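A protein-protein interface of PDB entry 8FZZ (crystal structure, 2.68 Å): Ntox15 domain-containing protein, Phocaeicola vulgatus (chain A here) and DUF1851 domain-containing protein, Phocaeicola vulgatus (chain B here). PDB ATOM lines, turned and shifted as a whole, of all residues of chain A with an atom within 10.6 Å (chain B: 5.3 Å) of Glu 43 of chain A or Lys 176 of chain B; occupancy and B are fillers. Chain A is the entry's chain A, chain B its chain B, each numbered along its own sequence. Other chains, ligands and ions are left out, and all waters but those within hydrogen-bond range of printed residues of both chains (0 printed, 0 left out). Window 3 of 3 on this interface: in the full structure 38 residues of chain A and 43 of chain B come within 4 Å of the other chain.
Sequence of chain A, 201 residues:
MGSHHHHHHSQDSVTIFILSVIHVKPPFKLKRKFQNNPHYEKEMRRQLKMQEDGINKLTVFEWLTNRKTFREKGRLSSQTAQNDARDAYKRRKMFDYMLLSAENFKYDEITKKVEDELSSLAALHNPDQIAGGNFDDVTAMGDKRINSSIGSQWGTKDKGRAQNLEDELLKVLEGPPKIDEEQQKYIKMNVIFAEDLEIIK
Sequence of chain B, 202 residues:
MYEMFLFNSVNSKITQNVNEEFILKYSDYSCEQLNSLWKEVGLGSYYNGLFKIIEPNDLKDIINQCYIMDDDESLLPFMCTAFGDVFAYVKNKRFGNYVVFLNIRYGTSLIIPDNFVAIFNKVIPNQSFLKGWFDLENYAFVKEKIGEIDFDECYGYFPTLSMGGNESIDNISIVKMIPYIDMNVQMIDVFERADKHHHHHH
NE2 of His 39 of chain A is in hydrogen-bond range of OE2 of Glu 43 of chain A (2.9 Å).
OD2 of Asp 152 of chain B lies within salt-bridge range of NZ of Lys 176 of chain B, at 3.5 Å.
N of Cys 154 of chain B is in hydrogen-bond range of O of Val 175 of chain B.
OE1 of Gln 47 of chain A sits close to O of Lys 176 of chain B.
Ile 178 of chain B touches Tyr 40 of chain A.
CA of Pro 179 of chain B touches OH of Tyr 40 of chain A (3.6 Å).
OE2 of Glu 43 of chain A touches CG of Lys 176 of chain B (3.6 Å).
Glu 43 of chain A touches Pro 179 of chain B (OE1 to CG, 3.5 Å).
Pro 179 of chain B touches Met 44 of chain A.
Gln 47 of chain A touches Val 175 of chain B.
NE2 of Gln 47 of chain A touches CA of Tyr 180 of chain B, at 3.6 Å.
Val 175 of chain B touches Met 50 of chain A (CG1 to CE, 3.7 Å).
Of the printed residues of chain B, Glu 43 of chain A touches Lys 176 and Pro 179.
Of chain A, only Glu 43 (3.6 Å) and Gln 47 (3.3 Å) come within 4 Å of Lys 176 of chain B.
No residue of chain A comes within 4 Å of Glu 153 of chain B.
No residue of chain A comes within 4 Å of Cys 154 of chain B.
Pro 179 of chain B touches just these residues of chain A: Tyr 40 (3.6 Å), Glu 43 (3.5 Å) and Met 44 (3.6 Å).
Printed residues of chain A within 4 Å of Tyr 180 of chain B: Gln 47.
Printed residues of chain B within 4 Å of Met 44 of chain A: Pro 179 (3.6 Å).
The nearest residue of chain A that does not touch Lys 176 of chain B is His 39 of chain A (5.0 Å).
Hydrophobic or aromatic side chains of chain A that line the printed part of chain B: Tyr 40, Met 44 and Met 50.
Along chain A the printed residues that touch a printed residue of chain B span positions 40 to 50.
Among the printed residues, 9 pairs touch across the chains.
Among the printed residues, no Asp or Glu carboxylate lies within 4 Å of a Lys or Arg side-chain nitrogen of the other chain.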
ATOM      1  N   LYS A  29     -34.928   4.442 -17.171  1.00  0.00           N
ATOM      2  CA  LYS A  29     -33.819   4.915 -17.991  1.00  0.00           C
ATOM      3  C   LYS A  29     -32.585   5.146 -17.122  1.00  0.00           C
ATOM      4  O   LYS A  29     -32.652   5.127 -15.892  1.00  0.00           O
ATOM      5  CB  LYS A  29     -34.222   6.190 -18.743  1.00  0.00           C
ATOM      6  CG  LYS A  29     -35.538   6.031 -19.536  1.00  0.00           C
ATOM      7  CD  LYS A  29     -35.875   7.258 -20.391  1.00  0.00           C
ATOM      8  CE  LYS A  29     -36.918   6.930 -21.458  1.00  0.00           C
ATOM      9  NZ  LYS A  29     -38.172   6.379 -20.867  1.00  0.00           N
ATOM     10  N   LEU A  30     -31.442   5.348 -17.775  1.00  0.00           N
ATOM     11  CA  LEU A  30     -30.179   5.536 -17.067  1.00  0.00           C
ATOM     12  C   LEU A  30     -29.297   6.519 -17.837  1.00  0.00           C
ATOM     13  O   LEU A  30     -29.359   6.604 -19.068  1.00  0.00           O
ATOM     14  CB  LEU A  30     -29.478   4.182 -16.849  1.00  0.00           C
ATOM     15  CG  LEU A  30     -28.045   4.084 -16.317  1.00  0.00           C
ATOM     16  CD1 LEU A  30     -27.865   4.812 -15.003  1.00  0.00           C
ATOM     17  CD2 LEU A  30     -27.666   2.619 -16.167  1.00  0.00           C
ATOM     18  N   PRO A  38     -20.418   3.868 -14.051  1.00  0.00           N
ATOM     19  CA  PRO A  38     -19.689   2.589 -14.075  1.00  0.00           C
ATOM     20  C   PRO A  38     -20.213   1.592 -13.042  1.00  0.00           C
ATOM     21  O   PRO A  38     -20.997   0.691 -13.354  1.00  0.00           O
ATOM     22  CB  PRO A  38     -18.248   3.004 -13.751  1.00  0.00           C
ATOM     23  CG  PRO A  38     -18.381   4.309 -12.944  1.00  0.00           C
ATOM     24  CD  PRO A  38     -19.754   4.890 -13.214  1.00  0.00           C
ATOM     25  N   HIS A  39     -19.744   1.768 -11.806  1.00  0.00           N
ATOM     26  CA  HIS A  39     -20.302   1.125 -10.625  1.00  0.00           C
ATOM     27  C   HIS A  39     -21.788   1.457 -10.439  1.00  0.00           C
ATOM     28  O   HIS A  39     -22.467   0.780  -9.659  1.00  0.00           O
ATOM     29  CB  HIS A  39     -19.434   1.574  -9.436  1.00  0.00           C
ATOM     30  CG  HIS A  39     -19.653   0.813  -8.163  1.00  0.00           C
ATOM     31  ND1 HIS A  39     -18.929   1.076  -7.018  1.00  0.00           N
ATOM     32  CD2 HIS A  39     -20.502  -0.194  -7.845  1.00  0.00           C
ATOM     33  CE1 HIS A  39     -19.324   0.267  -6.050  1.00  0.00           C
ATOM     34  NE2 HIS A  39     -20.280  -0.513  -6.525  1.00  0.00           N
ATOM     35  N   TYR A  40     -22.314   2.453 -11.168  1.00  0.00           N
ATOM     36  CA  TYR A  40     -23.699   2.903 -11.013  1.00  0.00           C
ATOM     37  C   TYR A  40     -24.693   1.948 -11.667  1.00  0.00           C
ATOM     38  O   TYR A  40     -25.693   1.564 -11.047  1.00  0.00           O
ATOM     39  CB  TYR A  40     -23.862   4.304 -11.609  1.00  0.00           C
ATOM     40  CG  TYR A  40     -25.090   5.054 -11.131  1.00  0.00           C
ATOM     41  CD1 TYR A  40     -25.058   5.800  -9.956  1.00  0.00           C
ATOM     42  CD2 TYR A  40     -26.283   5.024 -11.857  1.00  0.00           C
ATOM     43  CE1 TYR A  40     -26.178   6.496  -9.511  1.00  0.00           C
ATOM     44  CE2 TYR A  40     -27.415   5.714 -11.416  1.00  0.00           C
ATOM     45  CZ  TYR A  40     -27.350   6.446 -10.241  1.00  0.00           C
ATOM     46  OH  TYR A  40     -28.447   7.141  -9.784  1.00  0.00           O
ATOM     47  N   GLU A  41     -24.456   1.592 -12.936  1.00  0.00           N
ATOM     48  CA  GLU A  41     -25.342   0.668 -13.638  1.00  0.00           C
ATOM     49  C   GLU A  41     -25.415  -0.684 -12.939  1.00  0.00           C
ATOM     50  O   GLU A  41     -26.472  -1.325 -12.935  1.00  0.00           O
ATOM     51  CB  GLU A  41     -24.878   0.503 -15.085  1.00  0.00           C
ATOM     52  CG  GLU A  41     -23.492  -0.112 -15.237  1.00  0.00           C
ATOM     53  CD  GLU A  41     -23.010  -0.151 -16.685  1.00  0.00           C
ATOM     54  OE1 GLU A  41     -23.848  -0.027 -17.609  1.00  0.00           O
ATOM     55  OE2 GLU A  41     -21.780  -0.276 -16.894  1.00  0.00           O
ATOM     56  N   LYS A  42     -24.308  -1.128 -12.336  1.00  0.00           N
ATOM     57  CA  LYS A  42     -24.335  -2.342 -11.528  1.00  0.00           C
ATOM     58  C   LYS A  42     -25.336  -2.203 -10.392  1.00  0.00           C
ATOM     59  O   LYS A  42     -26.218  -3.052 -10.216  1.00  0.00           O
ATOM     60  CB  LYS A  42     -22.935  -2.633 -10.980  1.00  0.00           C
ATOM     61  CG  LYS A  42     -22.893  -3.738  -9.937  1.00  0.00           C
ATOM     62  CD  LYS A  42     -21.744  -3.560  -8.944  1.00  0.00           C
ATOM     63  CE  LYS A  42     -22.224  -3.011  -7.588  1.00  0.00           C
ATOM     64  NZ  LYS A  42     -23.487  -3.624  -7.029  1.00  0.00           N
ATOM     65  N   GLU A  43     -25.225  -1.110  -9.627  1.00  0.00           N
ATOM     66  CA  GLU A  43     -26.073  -0.909  -8.454  1.00  0.00           C
ATOM     67  C   GLU A  43     -27.548  -0.823  -8.815  1.00  0.00           C
ATOM     68  O   GLU A  43     -28.400  -1.163  -7.988  1.00  0.00           O
ATOM     69  CB  GLU A  43     -25.666   0.364  -7.717  1.00  0.00           C
ATOM     70  CG  GLU A  43     -24.758   0.174  -6.530  1.00  0.00           C
ATOM     71  CD  GLU A  43     -23.706   1.288  -6.418  1.00  0.00           C
ATOM     72  OE1 GLU A  43     -23.926   2.400  -6.953  1.00  0.00           O
ATOM     73  OE2 GLU A  43     -22.657   1.059  -5.775  1.00  0.00           O
ATOM     74  N   MET A  44     -27.873  -0.349 -10.017  1.00  0.00           N
ATOM     75  CA  MET A  44     -29.276  -0.118 -10.361  1.00  0.00           C
ATOM     76  C   MET A  44     -29.982  -1.295 -10.968  1.00  0.00           C
ATOM     77  O   MET A  44     -31.144  -1.531 -10.657  1.00  0.00           O
ATOM     78  CB  MET A  44     -29.441   1.064 -11.302  1.00  0.00           C
ATOM     79  CG  MET A  44     -29.577   2.331 -10.528  1.00  0.00           C
ATOM     80  SD  MET A  44     -30.970   3.417 -11.292  1.00  0.00           S
ATOM     81  CE  MET A  44     -32.470   2.294 -10.874  1.00  0.00           C
ATOM     82  N   ARG A  45     -29.314  -2.014 -11.868  1.00  0.00           N
ATOM     83  CA  ARG A  45     -29.797  -3.345 -12.199  1.00  0.00           C
ATOM     84  C   ARG A  45     -29.975  -4.154 -10.920  1.00  0.00           C
ATOM     85  O   ARG A  45     -31.045  -4.722 -10.675  1.00  0.00           O
ATOM     86  CB  ARG A  45     -28.831  -4.030 -13.163  1.00  0.00           C
ATOM     87  CG  ARG A  45     -28.464  -3.195 -14.376  1.00  0.00           C
ATOM     88  CD  ARG A  45     -27.972  -4.057 -15.538  1.00  0.00           C
ATOM     89  NE  ARG A  45     -28.946  -4.039 -16.618  1.00  0.00           N
ATOM     90  CZ  ARG A  45     -28.795  -3.366 -17.749  1.00  0.00           C
ATOM     91  NH1 ARG A  45     -27.668  -2.734 -18.030  1.00  0.00           N
ATOM     92  NH2 ARG A  45     -29.804  -3.318 -18.615  1.00  0.00           N
ATOM     93  N   ARG A  46     -28.952  -4.140 -10.056  1.00  0.00           N
ATOM     94  CA  ARG A  46     -28.997  -4.906  -8.814  1.00  0.00           C
ATOM     95  C   ARG A  46     -30.200  -4.533  -7.947  1.00  0.00           C
ATOM     96  O   ARG A  46     -30.878  -5.410  -7.400  1.00  0.00           O
ATOM     97  CB  ARG A  46     -27.701  -4.697  -8.037  1.00  0.00           C
ATOM     98  CG  ARG A  46     -27.603  -5.550  -6.790  1.00  0.00           C
ATOM     99  CD  ARG A  46     -27.098  -4.745  -5.613  1.00  0.00           C
ATOM    100  NE  ARG A  46     -26.976  -5.567  -4.415  1.00  0.00           N
ATOM    101  CZ  ARG A  46     -25.887  -5.621  -3.660  1.00  0.00           C
ATOM    102  NH1 ARG A  46     -24.804  -4.915  -3.957  1.00  0.00           N
ATOM    103  NH2 ARG A  46     -25.880  -6.413  -2.590  1.00  0.00           N
ATOM    104  N   GLN A  47     -30.476  -3.239  -7.805  1.00  0.00           N
ATOM    105  CA  GLN A  47     -31.543  -2.782  -6.925  1.00  0.00           C
ATOM    106  C   GLN A  47     -32.912  -2.883  -7.581  1.00  0.00           C
ATOM    107  O   GLN A  47     -33.921  -3.041  -6.884  1.00  0.00           O
ATOM    108  CB  GLN A  47     -31.272  -1.341  -6.506  1.00  0.00           C
ATOM    109  CG  GLN A  47     -30.306  -1.194  -5.358  1.00  0.00           C
ATOM    110  CD  GLN A  47     -30.377   0.189  -4.734  1.00  0.00           C
ATOM    111  OE1 GLN A  47     -29.500   0.593  -3.974  1.00  0.00           O
ATOM    112  NE2 GLN A  47     -31.427   0.928  -5.064  1.00  0.00           N
ATOM    113  N   LEU A  48     -32.976  -2.778  -8.907  1.00  0.00           N
ATOM    114  CA  LEU A  48     -34.254  -2.961  -9.589  1.00  0.00           C
ATOM    115  C   LEU A  48     -34.711  -4.416  -9.527  1.00  0.00           C
ATOM    116  O   LEU A  48     -35.910  -4.689  -9.388  1.00  0.00           O
ATOM    117  CB  LEU A  48     -34.160  -2.485 -11.039  1.00  0.00           C
ATOM    118  CG  LEU A  48     -34.268  -0.989 -11.306  1.00  0.00           C
ATOM    119  CD1 LEU A  48     -33.873  -0.689 -12.742  1.00  0.00           C
ATOM    120  CD2 LEU A  48     -35.663  -0.506 -11.035  1.00  0.00           C
ATOM    121  N   LYS A  49     -33.774  -5.367  -9.618  1.00  0.00           N
ATOM    122  CA  LYS A  49     -34.149  -6.771  -9.483  1.00  0.00           C
ATOM    123  C   LYS A  49     -34.701  -7.048  -8.093  1.00  0.00           C
ATOM    124  O   LYS A  49     -35.741  -7.703  -7.949  1.00  0.00           O
ATOM    125  CB  LYS A  49     -32.951  -7.673  -9.782  1.00  0.00           C
ATOM    126  CG  LYS A  49     -33.252  -9.171  -9.803  1.00  0.00           C
ATOM    127  CD  LYS A  49     -34.138  -9.572 -10.989  1.00  0.00           C
ATOM    128  CE  LYS A  49     -34.514 -11.064 -10.940  1.00  0.00           C
ATOM    129  NZ  LYS A  49     -35.682 -11.404 -11.819  1.00  0.00           N
ATOM    130  N   MET A  50     -34.031  -6.534  -7.064  1.00  0.00           N
ATOM    131  CA  MET A  50     -34.485  -6.652  -5.681  1.00  0.00           C
ATOM    132  C   MET A  50     -35.928  -6.175  -5.515  1.00  0.00           C
ATOM    133  O   MET A  50     -36.716  -6.796  -4.799  1.00  0.00           O
ATOM    134  CB  MET A  50     -33.577  -5.840  -4.761  1.00  0.00           C
ATOM    135  CG  MET A  50     -32.418  -6.583  -4.120  1.00  0.00           C
ATOM    136  SD  MET A  50     -31.019  -5.291  -3.567  1.00  0.00           S
ATOM    137  CE  MET A  50     -31.673  -4.816  -1.772  1.00  0.00           C
ATOM    138  N   GLN A  51     -36.250  -5.045  -6.160  1.00  0.00           N
ATOM    139  CA  GLN A  51     -37.630  -4.569  -6.206  1.00  0.00           C
ATOM    140  C   GLN A  51     -38.506  -5.542  -6.975  1.00  0.00           C
ATOM    141  O   GLN A  51     -39.591  -5.918  -6.517  1.00  0.00           O
ATOM    142  CB  GLN A  51     -37.697  -3.189  -6.868  1.00  0.00           C
ATOM    143  CG  GLN A  51     -36.983  -2.078  -6.142  1.00  0.00           C
ATOM    144  CD  GLN A  51     -37.874  -1.379  -5.118  1.00  0.00           C
ATOM    145  OE1 GLN A  51     -39.082  -1.210  -5.326  1.00  0.00           O
ATOM    146  NE2 GLN A  51     -37.270  -0.970  -3.996  1.00  0.00           N
ATOM    147  N   ALA A 194     -36.656  -4.949 -14.328  1.00  0.00           N
ATOM    148  CA  ALA A 194     -35.237  -4.693 -14.106  1.00  0.00           C
ATOM    149  C   ALA A 194     -34.397  -4.963 -15.356  1.00  0.00           C
ATOM    150  O   ALA A 194     -33.397  -4.274 -15.587  1.00  0.00           O
ATOM    151  CB  ALA A 194     -34.745  -5.525 -12.919  1.00  0.00           C
ATOM    152  N   LEU A 197     -33.887  -1.989 -18.246  1.00  0.00           N
ATOM    153  CA  LEU A 197     -33.229  -0.735 -17.899  1.00  0.00           C
ATOM    154  C   LEU A 197     -32.604  -0.140 -19.156  1.00  0.00           C
ATOM    155  O   LEU A 197     -31.555  -0.603 -19.619  1.00  0.00           O
ATOM    156  CB  LEU A 197     -32.157  -0.963 -16.839  1.00  0.00           C
ATOM    157  CG  LEU A 197     -31.255   0.234 -16.539  1.00  0.00           C
ATOM    158  CD1 LEU A 197     -32.000   1.283 -15.722  1.00  0.00           C
ATOM    159  CD2 LEU A 197     -29.986  -0.217 -15.820  1.00  0.00           C
ATOM    160  N   ILE A 199     -30.602   2.458 -21.593  1.00  0.00           N
ATOM    161  CA  ILE A 199     -29.358   3.231 -21.458  1.00  0.00           C
ATOM    162  C   ILE A 199     -29.324   4.378 -22.465  1.00  0.00           C
ATOM    163  O   ILE A 199     -29.286   5.552 -22.091  1.00  0.00           O
ATOM    164  CB  ILE A 199     -28.109   2.342 -21.627  1.00  0.00           C
ATOM    165  CG1 ILE A 199     -28.317   0.987 -20.948  1.00  0.00           C
ATOM    166  CG2 ILE A 199     -26.869   3.053 -21.076  1.00  0.00           C
ATOM    167  CD1 ILE A 199     -28.382   1.062 -19.438  1.00  0.00           C
ATOM    168  N   ASP B 150     -23.170   3.710   6.168  1.00  0.00           N
ATOM    169  CA  ASP B 150     -22.084   4.621   5.830  1.00  0.00           C
ATOM    170  C   ASP B 150     -22.718   5.921   5.355  1.00  0.00           C
ATOM    171  O   ASP B 150     -23.943   6.099   5.391  1.00  0.00           O
ATOM    172  CB  ASP B 150     -21.360   4.167   4.565  1.00  0.00           C
ATOM    173  CG  ASP B 150     -20.741   2.811   4.701  1.00  0.00           C
ATOM    174  OD1 ASP B 150     -20.730   2.275   5.831  1.00  0.00           O
ATOM    175  OD2 ASP B 150     -20.262   2.287   3.668  1.00  0.00           O
ATOM    176  N   ASP B 152     -22.697   7.015   2.087  1.00  0.00           N
ATOM    177  CA  ASP B 152     -23.340   6.868   0.793  1.00  0.00           C
ATOM    178  C   ASP B 152     -24.380   5.754   0.767  1.00  0.00           C
ATOM    179  O   ASP B 152     -24.815   5.357  -0.318  1.00  0.00           O
ATOM    180  CB  ASP B 152     -22.291   6.630  -0.292  1.00  0.00           C
ATOM    181  CG  ASP B 152     -21.544   5.324  -0.106  1.00  0.00           C
ATOM    182  OD1 ASP B 152     -21.384   4.887   1.062  1.00  0.00           O
ATOM    183  OD2 ASP B 152     -21.110   4.744  -1.136  1.00  0.00           O
ATOM    184  N   GLU B 153     -24.785   5.241   1.925  1.00  0.00           N
ATOM    185  CA  GLU B 153     -25.838   4.241   2.015  1.00  0.00           C
ATOM    186  C   GLU B 153     -27.085   4.862   2.633  1.00  0.00           C
ATOM    187  O   GLU B 153     -27.047   5.952   3.219  1.00  0.00           O
ATOM    188  CB  GLU B 153     -25.391   3.030   2.849  1.00  0.00           C
ATOM    189  CG  GLU B 153     -24.285   2.154   2.246  1.00  0.00           C
ATOM    190  CD  GLU B 153     -23.619   1.240   3.297  1.00  0.00           C
ATOM    191  OE1 GLU B 153     -23.757   1.527   4.510  1.00  0.00           O
ATOM    192  OE2 GLU B 153     -22.958   0.237   2.918  1.00  0.00           O
ATOM    193  N   CYS B 154     -28.202   4.146   2.503  1.00  0.00           N
ATOM    194  CA  CYS B 154     -29.430   4.504   3.207  1.00  0.00           C
ATOM    195  C   CYS B 154     -30.295   3.258   3.374  1.00  0.00           C
ATOM    196  O   CYS B 154     -29.983   2.176   2.860  1.00  0.00           O
ATOM    197  CB  CYS B 154     -30.202   5.598   2.464  1.00  0.00           C
ATOM    198  SG  CYS B 154     -31.056   4.971   0.967  1.00  0.00           S
ATOM    199  N   ILE B 174     -30.080  -2.018   3.824  1.00  0.00           N
ATOM    200  CA  ILE B 174     -29.073  -0.989   3.608  1.00  0.00           C
ATOM    201  C   ILE B 174     -28.568  -1.075   2.175  1.00  0.00           C
ATOM    202  O   ILE B 174     -27.977  -2.083   1.776  1.00  0.00           O
ATOM    203  CB  ILE B 174     -27.925  -1.155   4.603  1.00  0.00           C
ATOM    204  CG1 ILE B 174     -28.491  -1.253   6.018  1.00  0.00           C
ATOM    205  CG2 ILE B 174     -26.926  -0.035   4.448  1.00  0.00           C
ATOM    206  CD1 ILE B 174     -27.443  -1.338   7.108  1.00  0.00           C
ATOM    207  N   VAL B 175     -28.781  -0.008   1.396  1.00  0.00           N
ATOM    208  CA  VAL B 175     -28.401   0.029  -0.014  1.00  0.00           C
ATOM    209  C   VAL B 175     -27.785   1.386  -0.341  1.00  0.00           C
ATOM    210  O   VAL B 175     -27.844   2.334   0.447  1.00  0.00           O
ATOM    211  CB  VAL B 175     -29.596  -0.250  -0.955  1.00  0.00           C
ATOM    212  CG1 VAL B 175     -30.118  -1.660  -0.759  1.00  0.00           C
ATOM    213  CG2 VAL B 175     -30.703   0.770  -0.739  1.00  0.00           C
ATOM    214  N   LYS B 176     -27.198   1.471  -1.537  1.00  0.00           N
ATOM    215  CA  LYS B 176     -26.555   2.700  -1.983  1.00  0.00           C
ATOM    216  C   LYS B 176     -27.606   3.771  -2.232  1.00  0.00           C
ATOM    217  O   LYS B 176     -28.493   3.593  -3.079  1.00  0.00           O
ATOM    218  CB  LYS B 176     -25.744   2.451  -3.250  1.00  0.00           C
ATOM    219  CG  LYS B 176     -24.289   2.831  -3.114  1.00  0.00           C
ATOM    220  CD  LYS B 176     -23.620   2.009  -2.037  1.00  0.00           C
ATOM    221  CE  LYS B 176     -22.127   1.878  -2.286  1.00  0.00           C
ATOM    222  NZ  LYS B 176     -21.447   1.260  -1.106  1.00  0.00           N
ATOM    223  N   MET B 177     -27.496   4.884  -1.503  1.00  0.00           N
ATOM    224  CA  MET B 177     -28.433   6.007  -1.638  1.00  0.00           C
ATOM    225  C   MET B 177     -28.730   6.554  -3.028  1.00  0.00           C
ATOM    226  O   MET B 177     -29.899   6.580  -3.432  1.00  0.00           O
ATOM    227  CB  MET B 177     -27.984   7.198  -0.815  1.00  0.00           C
ATOM    228  CG  MET B 177     -29.179   7.968  -0.314  1.00  0.00           C
ATOM    229  SD  MET B 177     -28.648   9.391   0.860  1.00  0.00           S
ATOM    230  CE  MET B 177     -27.425  10.285  -0.381  1.00  0.00           C
ATOM    231  N   ILE B 178     -27.699   7.044  -3.725  1.00  0.00           N
ATOM    232  CA  ILE B 178     -27.931   7.767  -4.976  1.00  0.00           C
ATOM    233  C   ILE B 178     -28.733   6.931  -5.964  1.00  0.00           C
ATOM    234  O   ILE B 178     -29.755   7.424  -6.467  1.00  0.00           O
ATOM    235  CB  ILE B 178     -26.600   8.274  -5.558  1.00  0.00           C
ATOM    236  CG1 ILE B 178     -25.797   9.030  -4.498  1.00  0.00           C
ATOM    237  CG2 ILE B 178     -26.836   9.134  -6.785  1.00  0.00           C
ATOM    238  CD1 ILE B 178     -26.063  10.506  -4.458  1.00  0.00           C
ATOM    239  N   PRO B 179     -28.366   5.678  -6.265  1.00  0.00           N
ATOM    240  CA  PRO B 179     -29.233   4.881  -7.156  1.00  0.00           C
ATOM    241  C   PRO B 179     -30.622   4.640  -6.580  1.00  0.00           C
ATOM    242  O   PRO B 179     -31.591   4.558  -7.342  1.00  0.00           O
ATOM    243  CB  PRO B 179     -28.447   3.570  -7.340  1.00  0.00           C
ATOM    244  CG  PRO B 179     -27.041   3.908  -6.979  1.00  0.00           C
ATOM    245  CD  PRO B 179     -27.153   4.929  -5.882  1.00  0.00           C
ATOM    246  N   TYR B 180     -30.749   4.543  -5.254  1.00  0.00           N
ATOM    247  CA  TYR B 180     -32.067   4.402  -4.639  1.00  0.00           C
ATOM    248  C   TYR B 180     -32.949   5.613  -4.938  1.00  0.00           C
ATOM    249  O   TYR B 180     -34.074   5.469  -5.434  1.00  0.00           O
ATOM    250  CB  TYR B 180     -31.919   4.202  -3.130  1.00  0.00           C
ATOM    251  CG  TYR B 180     -33.218   3.936  -2.407  1.00  0.00           C
ATOM    252  CD1 TYR B 180     -34.000   2.836  -2.720  1.00  0.00           C
ATOM    253  CD2 TYR B 180     -33.655   4.776  -1.408  1.00  0.00           C
ATOM    254  CE1 TYR B 180     -35.188   2.588  -2.053  1.00  0.00           C
ATOM    255  CE2 TYR B 180     -34.838   4.540  -0.738  1.00  0.00           C
ATOM    256  CZ  TYR B 180     -35.599   3.451  -1.069  1.00  0.00           C
ATOM    257  OH  TYR B 180     -36.768   3.227  -0.390  1.00  0.00           O
